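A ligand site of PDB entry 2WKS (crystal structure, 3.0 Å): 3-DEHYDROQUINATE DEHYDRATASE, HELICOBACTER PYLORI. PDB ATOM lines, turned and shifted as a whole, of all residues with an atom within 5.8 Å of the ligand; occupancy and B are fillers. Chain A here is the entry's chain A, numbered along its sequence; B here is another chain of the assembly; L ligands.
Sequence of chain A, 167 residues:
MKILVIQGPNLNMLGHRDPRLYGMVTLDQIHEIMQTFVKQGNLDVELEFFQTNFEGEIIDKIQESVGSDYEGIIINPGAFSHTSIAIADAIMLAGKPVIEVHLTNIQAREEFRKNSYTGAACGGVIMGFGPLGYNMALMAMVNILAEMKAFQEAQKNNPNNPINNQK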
ATOM      1  N   PRO A   9     -14.122  -7.896   1.690  1.00  0.00           N
ATOM      2  CA  PRO A   9     -12.773  -8.155   1.222  1.00  0.00           C
ATOM      3  C   PRO A   9     -12.153  -7.003   0.428  1.00  0.00           C
ATOM      4  O   PRO A   9     -12.842  -6.287  -0.285  1.00  0.00           O
ATOM      5  CB  PRO A   9     -12.924  -9.397   0.341  1.00  0.00           C
ATOM      6  CG  PRO A   9     -14.365  -9.478   0.011  1.00  0.00           C
ATOM      7  CD  PRO A   9     -15.082  -8.894   1.178  1.00  0.00           C
ATOM      8  N   ASN A  10     -10.848  -6.814   0.593  1.00  0.00           N
ATOM      9  CA  ASN A  10     -10.056  -5.854  -0.183  1.00  0.00           C
ATOM     10  C   ASN A  10     -10.248  -4.393   0.117  1.00  0.00           C
ATOM     11  O   ASN A  10      -9.468  -3.570  -0.343  1.00  0.00           O
ATOM     12  CB  ASN A  10     -10.223  -6.078  -1.684  1.00  0.00           C
ATOM     13  CG  ASN A  10      -9.695  -7.404  -2.113  1.00  0.00           C
ATOM     14  OD1 ASN A  10      -8.551  -7.741  -1.818  1.00  0.00           O
ATOM     15  ND2 ASN A  10     -10.509  -8.174  -2.791  1.00  0.00           N
ATOM     16  N   LEU A  11     -11.275  -4.057   0.882  1.00  0.00           N
ATOM     17  CA  LEU A  11     -11.554  -2.661   1.201  1.00  0.00           C
ATOM     18  C   LEU A  11     -10.507  -2.033   2.111  1.00  0.00           C
ATOM     19  O   LEU A  11     -10.338  -0.812   2.122  1.00  0.00           O
ATOM     20  CB  LEU A  11     -12.943  -2.512   1.785  1.00  0.00           C
ATOM     21  CG  LEU A  11     -14.033  -2.577   0.725  1.00  0.00           C
ATOM     22  CD1 LEU A  11     -15.339  -2.895   1.390  1.00  0.00           C
ATOM     23  CD2 LEU A  11     -14.092  -1.275  -0.042  1.00  0.00           C
ATOM     24  N   MET A  13      -7.486  -2.324   1.495  1.00  0.00           N
ATOM     25  CA  MET A  13      -6.410  -1.896   0.589  1.00  0.00           C
ATOM     26  C   MET A  13      -6.672  -0.530  -0.028  1.00  0.00           C
ATOM     27  O   MET A  13      -5.845   0.026  -0.749  1.00  0.00           O
ATOM     28  CB  MET A  13      -6.152  -2.927  -0.512  1.00  0.00           C
ATOM     29  CG  MET A  13      -5.679  -4.254   0.003  1.00  0.00           C
ATOM     30  SD  MET A  13      -4.185  -4.160   1.010  1.00  0.00           S
ATOM     31  CE  MET A  13      -2.960  -3.659  -0.189  1.00  0.00           C
ATOM     32  N   LEU A  14      -7.823   0.028   0.265  1.00  0.00           N
ATOM     33  CA  LEU A  14      -8.187   1.305  -0.320  1.00  0.00           C
ATOM     34  C   LEU A  14      -7.132   2.365  -0.146  1.00  0.00           C
ATOM     35  O   LEU A  14      -6.467   2.452   0.892  1.00  0.00           O
ATOM     36  CB  LEU A  14      -9.468   1.830   0.312  1.00  0.00           C
ATOM     37  CG  LEU A  14     -10.732   1.357  -0.354  1.00  0.00           C
ATOM     38  CD1 LEU A  14     -11.857   1.955   0.415  1.00  0.00           C
ATOM     39  CD2 LEU A  14     -10.737   1.775  -1.814  1.00  0.00           C
ATOM     40  N   PRO A  19      -5.225   3.056  -6.438  1.00  0.00           N
ATOM     41  CA  PRO A  19      -5.476   2.199  -7.610  1.00  0.00           C
ATOM     42  C   PRO A  19      -6.723   2.591  -8.473  1.00  0.00           C
ATOM     43  O   PRO A  19      -7.508   1.725  -8.902  1.00  0.00           O
ATOM     44  CB  PRO A  19      -5.596   0.779  -6.990  1.00  0.00           C
ATOM     45  CG  PRO A  19      -5.145   0.942  -5.522  1.00  0.00           C
ATOM     46  CD  PRO A  19      -5.571   2.349  -5.193  1.00  0.00           C
ATOM     47  N   LEU A  21      -9.840   3.303  -9.670  1.00  0.00           N
ATOM     48  CA  LEU A  21     -11.321   3.049  -9.673  1.00  0.00           C
ATOM     49  C   LEU A  21     -12.065   3.473  -8.378  1.00  0.00           C
ATOM     50  O   LEU A  21     -13.135   4.083  -8.427  1.00  0.00           O
ATOM     51  CB  LEU A  21     -11.636   1.543  -9.960  1.00  0.00           C
ATOM     52  CG  LEU A  21     -10.763   0.554 -10.798  1.00  0.00           C
ATOM     53  CD1 LEU A  21      -9.652  -0.158  -9.971  1.00  0.00           C
ATOM     54  CD2 LEU A  21     -11.614  -0.484 -11.576  1.00  0.00           C
ATOM     55  N   TYR A  22     -11.455   3.137  -7.244  1.00  0.00           N
ATOM     56  CA  TYR A  22     -12.039   3.269  -5.906  1.00  0.00           C
ATOM     57  C   TYR A  22     -11.630   4.605  -5.226  1.00  0.00           C
ATOM     58  O   TYR A  22     -12.355   5.117  -4.374  1.00  0.00           O
ATOM     59  CB  TYR A  22     -11.713   2.021  -5.016  1.00  0.00           C
ATOM     60  CG  TYR A  22     -12.194   0.684  -5.599  1.00  0.00           C
ATOM     61  CD1 TYR A  22     -11.474   0.027  -6.604  1.00  0.00           C
ATOM     62  CD2 TYR A  22     -13.381   0.082  -5.162  1.00  0.00           C
ATOM     63  CE1 TYR A  22     -11.910  -1.176  -7.178  1.00  0.00           C
ATOM     64  CE2 TYR A  22     -13.826  -1.133  -5.721  1.00  0.00           C
ATOM     65  CZ  TYR A  22     -13.079  -1.755  -6.738  1.00  0.00           C
ATOM     66  OH  TYR A  22     -13.460  -2.964  -7.308  1.00  0.00           O
ATOM     67  N   ASN A  76     -20.652  -3.049   3.359  1.00  0.00           N
ATOM     68  CA  ASN A  76     -20.204  -3.107   2.004  1.00  0.00           C
ATOM     69  C   ASN A  76     -19.537  -4.448   1.848  1.00  0.00           C
ATOM     70  O   ASN A  76     -18.371  -4.572   2.232  1.00  0.00           O
ATOM     71  CB  ASN A  76     -19.203  -2.009   1.703  1.00  0.00           C
ATOM     72  CG  ASN A  76     -18.645  -2.117   0.309  1.00  0.00           C
ATOM     73  OD1 ASN A  76     -18.775  -3.156  -0.316  1.00  0.00           O
ATOM     74  ND2 ASN A  76     -18.036  -1.058  -0.189  1.00  0.00           N
ATOM     75  N   PRO A  77     -20.260  -5.459   1.325  1.00  0.00           N
ATOM     76  CA  PRO A  77     -19.736  -6.812   1.267  1.00  0.00           C
ATOM     77  C   PRO A  77     -18.682  -6.984   0.202  1.00  0.00           C
ATOM     78  O   PRO A  77     -18.163  -8.080   0.045  1.00  0.00           O
ATOM     79  CB  PRO A  77     -20.959  -7.648   0.887  1.00  0.00           C
ATOM     80  CG  PRO A  77     -22.130  -6.768   1.066  1.00  0.00           C
ATOM     81  CD  PRO A  77     -21.625  -5.400   0.781  1.00  0.00           C
ATOM     82  N   GLY A  78     -18.352  -5.925  -0.544  1.00  0.00           N
ATOM     83  CA  GLY A  78     -17.335  -6.007  -1.605  1.00  0.00           C
ATOM     84  C   GLY A  78     -17.683  -7.081  -2.612  1.00  0.00           C
ATOM     85  O   GLY A  78     -18.852  -7.345  -2.879  1.00  0.00           O
ATOM     86  N   ALA A  79     -16.670  -7.730  -3.162  1.00  0.00           N
ATOM     87  CA  ALA A  79     -16.925  -8.711  -4.205  1.00  0.00           C
ATOM     88  C   ALA A  79     -17.845  -9.843  -3.760  1.00  0.00           C
ATOM     89  O   ALA A  79     -18.345 -10.568  -4.598  1.00  0.00           O
ATOM     90  CB  ALA A  79     -15.619  -9.274  -4.762  1.00  0.00           C
ATOM     91  N   PHE A  80     -18.074 -10.012  -2.458  1.00  0.00           N
ATOM     92  CA  PHE A  80     -19.008 -11.040  -1.996  1.00  0.00           C
ATOM     93  C   PHE A  80     -20.474 -10.681  -2.286  1.00  0.00           C
ATOM     94  O   PHE A  80     -21.359 -11.535  -2.262  1.00  0.00           O
ATOM     95  CB  PHE A  80     -18.872 -11.288  -0.510  1.00  0.00           C
ATOM     96  CG  PHE A  80     -17.576 -11.890  -0.096  1.00  0.00           C
ATOM     97  CD1 PHE A  80     -16.881 -12.730  -0.947  1.00  0.00           C
ATOM     98  CD2 PHE A  80     -17.074 -11.660   1.183  1.00  0.00           C
ATOM     99  CE1 PHE A  80     -15.665 -13.310  -0.540  1.00  0.00           C
ATOM    100  CE2 PHE A  80     -15.862 -12.216   1.593  1.00  0.00           C
ATOM    101  CZ  PHE A  80     -15.162 -13.043   0.741  1.00  0.00           C
ATOM    102  N   SER A  81     -20.742  -9.409  -2.531  1.00  0.00           N
ATOM    103  CA  SER A  81     -22.089  -8.988  -2.837  1.00  0.00           C
ATOM    104  C   SER A  81     -22.644  -9.850  -3.928  1.00  0.00           C
ATOM    105  O   SER A  81     -23.808 -10.245  -3.889  1.00  0.00           O
ATOM    106  CB  SER A  81     -22.097  -7.547  -3.308  1.00  0.00           C
ATOM    107  OG  SER A  81     -21.322  -6.751  -2.443  1.00  0.00           O
ATOM    108  N   HIS A  82     -21.809 -10.165  -4.909  1.00  0.00           N
ATOM    109  CA  HIS A  82     -22.271 -10.771  -6.149  1.00  0.00           C
ATOM    110  C   HIS A  82     -22.378 -12.262  -6.077  1.00  0.00           C
ATOM    111  O   HIS A  82     -23.088 -12.862  -6.866  1.00  0.00           O
ATOM    112  CB  HIS A  82     -21.336 -10.387  -7.290  1.00  0.00           C
ATOM    113  CG  HIS A  82     -20.859  -8.977  -7.222  1.00  0.00           C
ATOM    114  ND1 HIS A  82     -21.729  -7.905  -7.266  1.00  0.00           N
ATOM    115  CD2 HIS A  82     -19.623  -8.462  -7.097  1.00  0.00           C
ATOM    116  CE1 HIS A  82     -21.031  -6.782  -7.165  1.00  0.00           C
ATOM    117  NE2 HIS A  82     -19.757  -7.090  -7.065  1.00  0.00           N
ATOM    118  N   VAL A 101     -23.777  -0.564   1.087  1.00  0.00           N
ATOM    119  CA  VAL A 101     -23.099   0.556   0.437  1.00  0.00           C
ATOM    120  C   VAL A 101     -22.080   0.037  -0.543  1.00  0.00           C
ATOM    121  O   VAL A 101     -21.440  -0.981  -0.290  1.00  0.00           O
ATOM    122  CB  VAL A 101     -22.408   1.487   1.472  1.00  0.00           C
ATOM    123  CG1 VAL A 101     -21.609   2.621   0.785  1.00  0.00           C
ATOM    124  CG2 VAL A 101     -23.413   2.031   2.468  1.00  0.00           C
ATOM    125  N   HIS A 102     -21.935   0.717  -1.670  1.00  0.00           N
ATOM    126  CA  HIS A 102     -20.818   0.519  -2.568  1.00  0.00           C
ATOM    127  C   HIS A 102     -20.235   1.861  -2.966  1.00  0.00           C
ATOM    128  O   HIS A 102     -20.950   2.791  -3.344  1.00  0.00           O
ATOM    129  CB  HIS A 102     -21.266  -0.192  -3.826  1.00  0.00           C
ATOM    130  CG  HIS A 102     -21.925  -1.495  -3.579  1.00  0.00           C
ATOM    131  ND1 HIS A 102     -21.209  -2.647  -3.326  1.00  0.00           N
ATOM    132  CD2 HIS A 102     -23.231  -1.844  -3.571  1.00  0.00           C
ATOM    133  CE1 HIS A 102     -22.055  -3.656  -3.168  1.00  0.00           C
ATOM    134  NE2 HIS A 102     -23.292  -3.197  -3.309  1.00  0.00           N
ATOM    135  N   LEU A 103     -18.916   1.936  -2.885  1.00  0.00           N
ATOM    136  CA  LEU A 103     -18.171   3.064  -3.408  1.00  0.00           C
ATOM    137  C   LEU A 103     -18.500   3.301  -4.873  1.00  0.00           C
ATOM    138  O   LEU A 103     -18.874   4.398  -5.246  1.00  0.00           O
ATOM    139  CB  LEU A 103     -16.665   2.861  -3.225  1.00  0.00           C
ATOM    140  CG  LEU A 103     -16.163   2.694  -1.790  1.00  0.00           C
ATOM    141  CD1 LEU A 103     -14.834   2.083  -1.830  1.00  0.00           C
ATOM    142  CD2 LEU A 103     -16.084   4.035  -1.038  1.00  0.00           C
ATOM    143  N   THR A 104     -18.375   2.282  -5.703  1.00  0.00           N
ATOM    144  CA  THR A 104     -18.531   2.470  -7.134  1.00  0.00           C
ATOM    145  C   THR A 104     -19.959   2.133  -7.565  1.00  0.00           C
ATOM    146  O   THR A 104     -20.678   1.454  -6.829  1.00  0.00           O
ATOM    147  CB  THR A 104     -17.573   1.565  -7.875  1.00  0.00           C
ATOM    148  OG1 THR A 104     -17.957   0.211  -7.658  1.00  0.00           O
ATOM    149  CG2 THR A 104     -16.151   1.734  -7.353  1.00  0.00           C
ATOM    150  N   ASN A 105     -20.378   2.569  -8.750  1.00  0.00           N
ATOM    151  CA  ASN A 105     -21.709   2.215  -9.275  1.00  0.00           C
ATOM    152  C   ASN A 105     -21.699   0.829  -9.886  1.00  0.00           C
ATOM    153  O   ASN A 105     -21.378   0.695 -11.069  1.00  0.00           O
ATOM    154  CB  ASN A 105     -22.155   3.247 -10.324  1.00  0.00           C
ATOM    155  CG  ASN A 105     -23.632   3.070 -10.772  1.00  0.00           C
ATOM    156  OD1 ASN A 105     -24.255   2.024 -10.581  1.00  0.00           O
ATOM    157  ND2 ASN A 105     -24.169   4.131 -11.374  1.00  0.00           N
ATOM    158  N   ILE A 106     -22.068  -0.199  -9.127  1.00  0.00           N
ATOM    159  CA  ILE A 106     -21.946  -1.572  -9.636  1.00  0.00           C
ATOM    160  C   ILE A 106     -22.863  -1.908 -10.817  1.00  0.00           C
ATOM    161  O   ILE A 106     -22.670  -2.926 -11.498  1.00  0.00           O
ATOM    162  CB  ILE A 106     -22.033  -2.644  -8.530  1.00  0.00           C
ATOM    163  CG1 ILE A 106     -23.366  -2.603  -7.807  1.00  0.00           C
ATOM    164  CG2 ILE A 106     -20.904  -2.468  -7.557  1.00  0.00           C
ATOM    165  CD1 ILE A 106     -23.616  -3.808  -6.907  1.00  0.00           C
ATOM    166  N   ARG A 109     -20.563  -1.502 -14.219  1.00  0.00           N
ATOM    167  CA  ARG A 109     -19.311  -2.253 -14.369  1.00  0.00           C
ATOM    168  C   ARG A 109     -19.607  -3.565 -15.083  1.00  0.00           C
ATOM    169  O   ARG A 109     -20.648  -3.690 -15.705  1.00  0.00           O
ATOM    170  CB  ARG A 109     -18.600  -2.432 -13.021  1.00  0.00           C
ATOM    171  CG  ARG A 109     -18.151  -1.112 -12.401  1.00  0.00           C
ATOM    172  CD  ARG A 109     -17.543  -1.305 -11.032  1.00  0.00           C
ATOM    173  NE  ARG A 109     -16.301  -2.080 -11.091  1.00  0.00           N
ATOM    174  CZ  ARG A 109     -15.560  -2.413 -10.027  1.00  0.00           C
ATOM    175  NH1 ARG A 109     -15.921  -2.028  -8.797  1.00  0.00           N
ATOM    176  NH2 ARG A 109     -14.436  -3.117 -10.180  1.00  0.00           N
ATOM    177  N   ARG A 113     -20.769  -8.139 -11.860  1.00  0.00           N
ATOM    178  CA  ARG A 113     -20.897  -7.246 -10.696  1.00  0.00           C
ATOM    179  C   ARG A 113     -22.274  -6.584 -10.544  1.00  0.00           C
ATOM    180  O   ARG A 113     -22.522  -5.907  -9.539  1.00  0.00           O
ATOM    181  CB  ARG A 113     -19.824  -6.130 -10.728  1.00  0.00           C
ATOM    182  CG  ARG A 113     -18.411  -6.583 -10.448  1.00  0.00           C
ATOM    183  CD  ARG A 113     -17.420  -5.405 -10.411  1.00  0.00           C
ATOM    184  NE  ARG A 113     -16.027  -5.861 -10.528  1.00  0.00           N
ATOM    185  CZ  ARG A 113     -15.275  -6.237  -9.506  1.00  0.00           C
ATOM    186  NH1 ARG A 113     -15.739  -6.221  -8.270  1.00  0.00           N
ATOM    187  NH2 ARG A 113     -14.047  -6.641  -9.707  1.00  0.00           N
ATOM    188  N   TYR A 134     -21.331   6.262   2.562  1.00  0.00           N
ATOM    189  CA  TYR A 134     -21.415   5.746   3.925  1.00  0.00           C
ATOM    190  C   TYR A 134     -22.137   6.711   4.847  1.00  0.00           C
ATOM    191  O   TYR A 134     -22.865   6.273   5.748  1.00  0.00           O
ATOM    192  CB  TYR A 134     -20.028   5.430   4.462  1.00  0.00           C
ATOM    193  CG  TYR A 134     -19.395   4.196   3.874  1.00  0.00           C
ATOM    194  CD1 TYR A 134     -18.610   4.275   2.744  1.00  0.00           C
ATOM    195  CD2 TYR A 134     -19.599   2.943   4.458  1.00  0.00           C
ATOM    196  CE1 TYR A 134     -18.018   3.133   2.204  1.00  0.00           C
ATOM    197  CE2 TYR A 134     -19.007   1.795   3.941  1.00  0.00           C
ATOM    198  CZ  TYR A 134     -18.225   1.890   2.808  1.00  0.00           C
ATOM    199  OH  TYR A 134     -17.642   0.753   2.294  1.00  0.00           O
ATOM    200  N   ILE B  85     -14.522 -13.774  -7.354  1.00  0.00           N
ATOM    201  CA  ILE B  85     -14.269 -12.414  -7.787  1.00  0.00           C
ATOM    202  C   ILE B  85     -13.380 -11.731  -6.734  1.00  0.00           C
ATOM    203  O   ILE B  85     -12.498 -10.929  -7.068  1.00  0.00           O
ATOM    204  CB  ILE B  85     -15.594 -11.659  -7.948  1.00  0.00           C
ATOM    205  CG1 ILE B  85     -16.490 -12.316  -8.985  1.00  0.00           C
ATOM    206  CG2 ILE B  85     -15.356 -10.232  -8.336  1.00  0.00           C
ATOM    207  CD1 ILE B  85     -17.977 -12.005  -8.817  1.00  0.00           C
ATOM    208  N   ASP B  89     -10.077  -9.646  -7.450  1.00  0.00           N
ATOM    209  CA  ASP B  89      -9.828  -8.236  -7.111  1.00  0.00           C
ATOM    210  C   ASP B  89      -8.494  -8.067  -6.385  1.00  0.00           C
ATOM    211  O   ASP B  89      -7.707  -7.176  -6.710  1.00  0.00           O
ATOM    212  CB  ASP B  89     -10.984  -7.647  -6.298  1.00  0.00           C
ATOM    213  CG  ASP B  89     -12.203  -7.319  -7.150  1.00  0.00           C
ATOM    214  OD1 ASP B  89     -12.110  -7.438  -8.401  1.00  0.00           O
ATOM    215  OD2 ASP B  89     -13.257  -6.963  -6.562  1.00  0.00           O
ATOM    216  N   ALA B  90      -8.252  -8.925  -5.406  1.00  0.00           N
ATOM    217  CA  ALA B  90      -6.982  -8.928  -4.676  1.00  0.00           C
ATOM    218  C   ALA B  90      -5.809  -9.021  -5.624  1.00  0.00           C
ATOM    219  O   ALA B  90      -4.868  -8.274  -5.449  1.00  0.00           O
ATOM    220  CB  ALA B  90      -6.938 -10.053  -3.700  1.00  0.00           C
ATOM    221  N   MET B  92      -5.771  -8.073  -8.770  1.00  0.00           N
ATOM    222  CA  MET B  92      -5.684  -6.832  -9.503  1.00  0.00           C
ATOM    223  C   MET B  92      -5.018  -5.710  -8.722  1.00  0.00           C
ATOM    224  O   MET B  92      -4.368  -4.843  -9.306  1.00  0.00           O
ATOM    225  CB  MET B  92      -7.040  -6.398  -9.979  1.00  0.00           C
ATOM    226  CG  MET B  92      -7.203  -6.503 -11.467  1.00  0.00           C
ATOM    227  SD  MET B  92      -8.971  -6.504 -11.691  1.00  0.00           S
ATOM    228  CE  MET B  92      -9.537  -4.888 -11.092  1.00  0.00           C
ATOM    229  N   LEU B  93      -5.178  -5.708  -7.408  1.00  0.00           N
ATOM    230  CA  LEU B  93      -4.546  -4.677  -6.595  1.00  0.00           C
ATOM    231  C   LEU B  93      -3.170  -5.050  -6.054  1.00  0.00           C
ATOM    232  O   LEU B  93      -2.594  -4.316  -5.260  1.00  0.00           O
ATOM    233  CB  LEU B  93      -5.448  -4.258  -5.426  1.00  0.00           C
ATOM    234  CG  LEU B  93      -5.924  -5.300  -4.399  1.00  0.00           C
ATOM    235  CD1 LEU B  93      -4.852  -5.735  -3.355  1.00  0.00           C
ATOM    236  CD2 LEU B  93      -7.196  -4.784  -3.711  1.00  0.00           C
HETATM  237  C1  LIG L   1     -11.744  -3.604  -4.558  1.00  0.00           C
HETATM  238  C2  LIG L   1     -10.529  -3.131  -4.922  1.00  0.00           C
HETATM  239  C3  LIG L   1      -9.748  -3.534  -6.027  1.00  0.00           C
HETATM  240  C4  LIG L   1      -8.511  -2.953  -6.287  1.00  0.00           C
HETATM  241  C5  LIG L   1      -8.019  -1.953  -5.433  1.00  0.00           C
HETATM  242  C6  LIG L   1      -8.768  -1.524  -4.329  1.00  0.00           C
HETATM  243  C7  LIG L   1     -10.019  -2.115  -4.072  1.00  0.00           C
HETATM  244  S1  LIG L   1     -11.200  -1.899  -2.867  1.00  0.00           S
HETATM  245  C8  LIG L   1     -12.260  -3.043  -3.465  1.00  0.00           C
HETATM  246  C9  LIG L   1     -13.487  -3.364  -2.924  1.00  0.00           C
HETATM  247  O1  LIG L   1     -14.268  -4.336  -3.614  1.00  0.00           O
HETATM  248  C10 LIG L   1     -15.465  -3.969  -4.156  1.00  0.00           C
HETATM  249  C11 LIG L   1     -16.323  -3.022  -3.577  1.00  0.00           C
HETATM  250  C12 LIG L   1     -17.582  -2.632  -4.083  1.00  0.00           C
HETATM  251  C13 LIG L   1     -17.644  -1.106  -4.034  1.00  0.00           C
HETATM  252  O2  LIG L   1     -17.557  -0.595  -2.880  1.00  0.00           O
HETATM  253  O3  LIG L   1     -17.769  -0.467  -5.116  1.00  0.00           O
HETATM  254  O4  LIG L   1     -18.626  -3.127  -3.239  1.00  0.00           O
HETATM  255  C14 LIG L   1     -17.841  -3.175  -5.499  1.00  0.00           C
HETATM  256  C15 LIG L   1     -17.416  -4.658  -5.570  1.00  0.00           C
HETATM  257  O5  LIG L   1     -17.772  -5.183  -6.833  1.00  0.00           O
HETATM  258  C16 LIG L   1     -15.902  -4.759  -5.399  1.00  0.00           C
HETATM  259  O6  LIG L   1     -15.467  -6.118  -5.230  1.00  0.00           O
HETATM  260  C17 LIG L   1      -7.728  -3.450  -7.514  1.00  0.00           C
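OD2 of Asp 89 of chain B sits at hydrogen-bond distance from O6 of the ligand, at 2.7 Å.
OG1 of Thr 104 is in hydrogen-bond range of O3 of the ligand (2.6 Å).
An oxygen (O5) of the ligand sits at hydrogen-bond distance from a ring nitrogen (NE2) of His 82 (2.8 Å).
The backbone NH (N) of Thr 104 is in hydrogen-bond range of an oxygen (O3) of the ligand (2.9 Å).
An oxygen (O2) of the ligand is in hydrogen-bond range of the backbone NH (N) of Leu 103 (2.9 Å).
A ring nitrogen (ND1) of His 102 sits at hydrogen-bond distance from an oxygen (O4) of the ligand.
An oxygen (O5) of the ligand is in hydrogen-bond range of the guanidinium group (NH1) of Arg 113, at 2.7 Å.
The side-chain amide nitrogen (ND2) of Asn 76 is in hydrogen-bond range of an oxygen (O2) of the ligand, at 2.8 Å.
The backbone NH (N) of Ala 79 is in hydrogen-bond range of an oxygen (O6) of the ligand.
OH of Tyr 134 sits at hydrogen-bond distance from ND2 of Asn 76.
The backbone carbonyl oxygen (O) of Arg 113 lies close to a ring nitrogen (ND1) of His 82, at 3.1 Å.
The side-chain hydroxyl (OG) of Ser 81 sits at hydrogen-bond distance from the backbone carbonyl oxygen (O) of Gly 78 (2.6 Å).
The backbone NH of Gly 78 sits at hydrogen-bond distance from the side-chain amide oxygen of Asn 76 (2.8 Å).
The side-chain amide nitrogen of Asn 76 sits close to the backbone carbonyl oxygen of Val 101.
The guanidinium group of Arg 113 lies within salt-bridge range of the side-chain carboxylate of Asp 89 of chain B, at 2.5 Å.
OH of Tyr 22 lies within hydrogen-bond range of NH1 of Arg 109 (3.0 Å).
The side-chain hydroxyl (OG1) of Thr 104 lies within hydrogen-bond range of the guanidinium group (NH1) of Arg 109 (3.2 Å).
The backbone carbonyl oxygen of Asn 10 lies close to a sulfur (S1) of the ligand (3.5 Å).
Pro 9 touches the ligand (O to C9, 3.99 Å).
CD2 of Leu 11 touches C9 of the ligand (3.6 Å).
CD2 of Leu 14 touches S1 of the ligand (3.8 Å).
Pro 19 touches the ligand.
Tyr 22 touches the ligand (CZ to C1, 3.2 Å).
CA of Gly 78 touches O4 of the ligand, 3.6 Å away.
CG2 of Ile 106 touches C14 of the ligand, 3.8 Å away.
Arg 109 touches the ligand (NH1 to C14, 3.98 Å).
Met 92 of chain B touches the ligand.
CB of Leu 93 of chain B touches C17 of the ligand, at 3.2 Å.
Hydrophobic or aromatic side chains that line the ligand: Leu 11, Leu 14, Pro 19, Tyr 22, Ala 79, His 82, His 102, Leu 103, Ile 106, Met 92 of chain B and Leu 93 of chain B.
19 residues have an atom within 4 Å of the ligand: Pro 9, Asn 10, Leu 11, Leu 14, Pro 19, Tyr 22, Asn 76, Gly 78, Ala 79, His 82, His 102, Leu 103, Thr 104, Ile 106, Arg 109, Arg 113, Asp 89 of chain B, Met 92 of chain B and Leu 93 of chain B.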
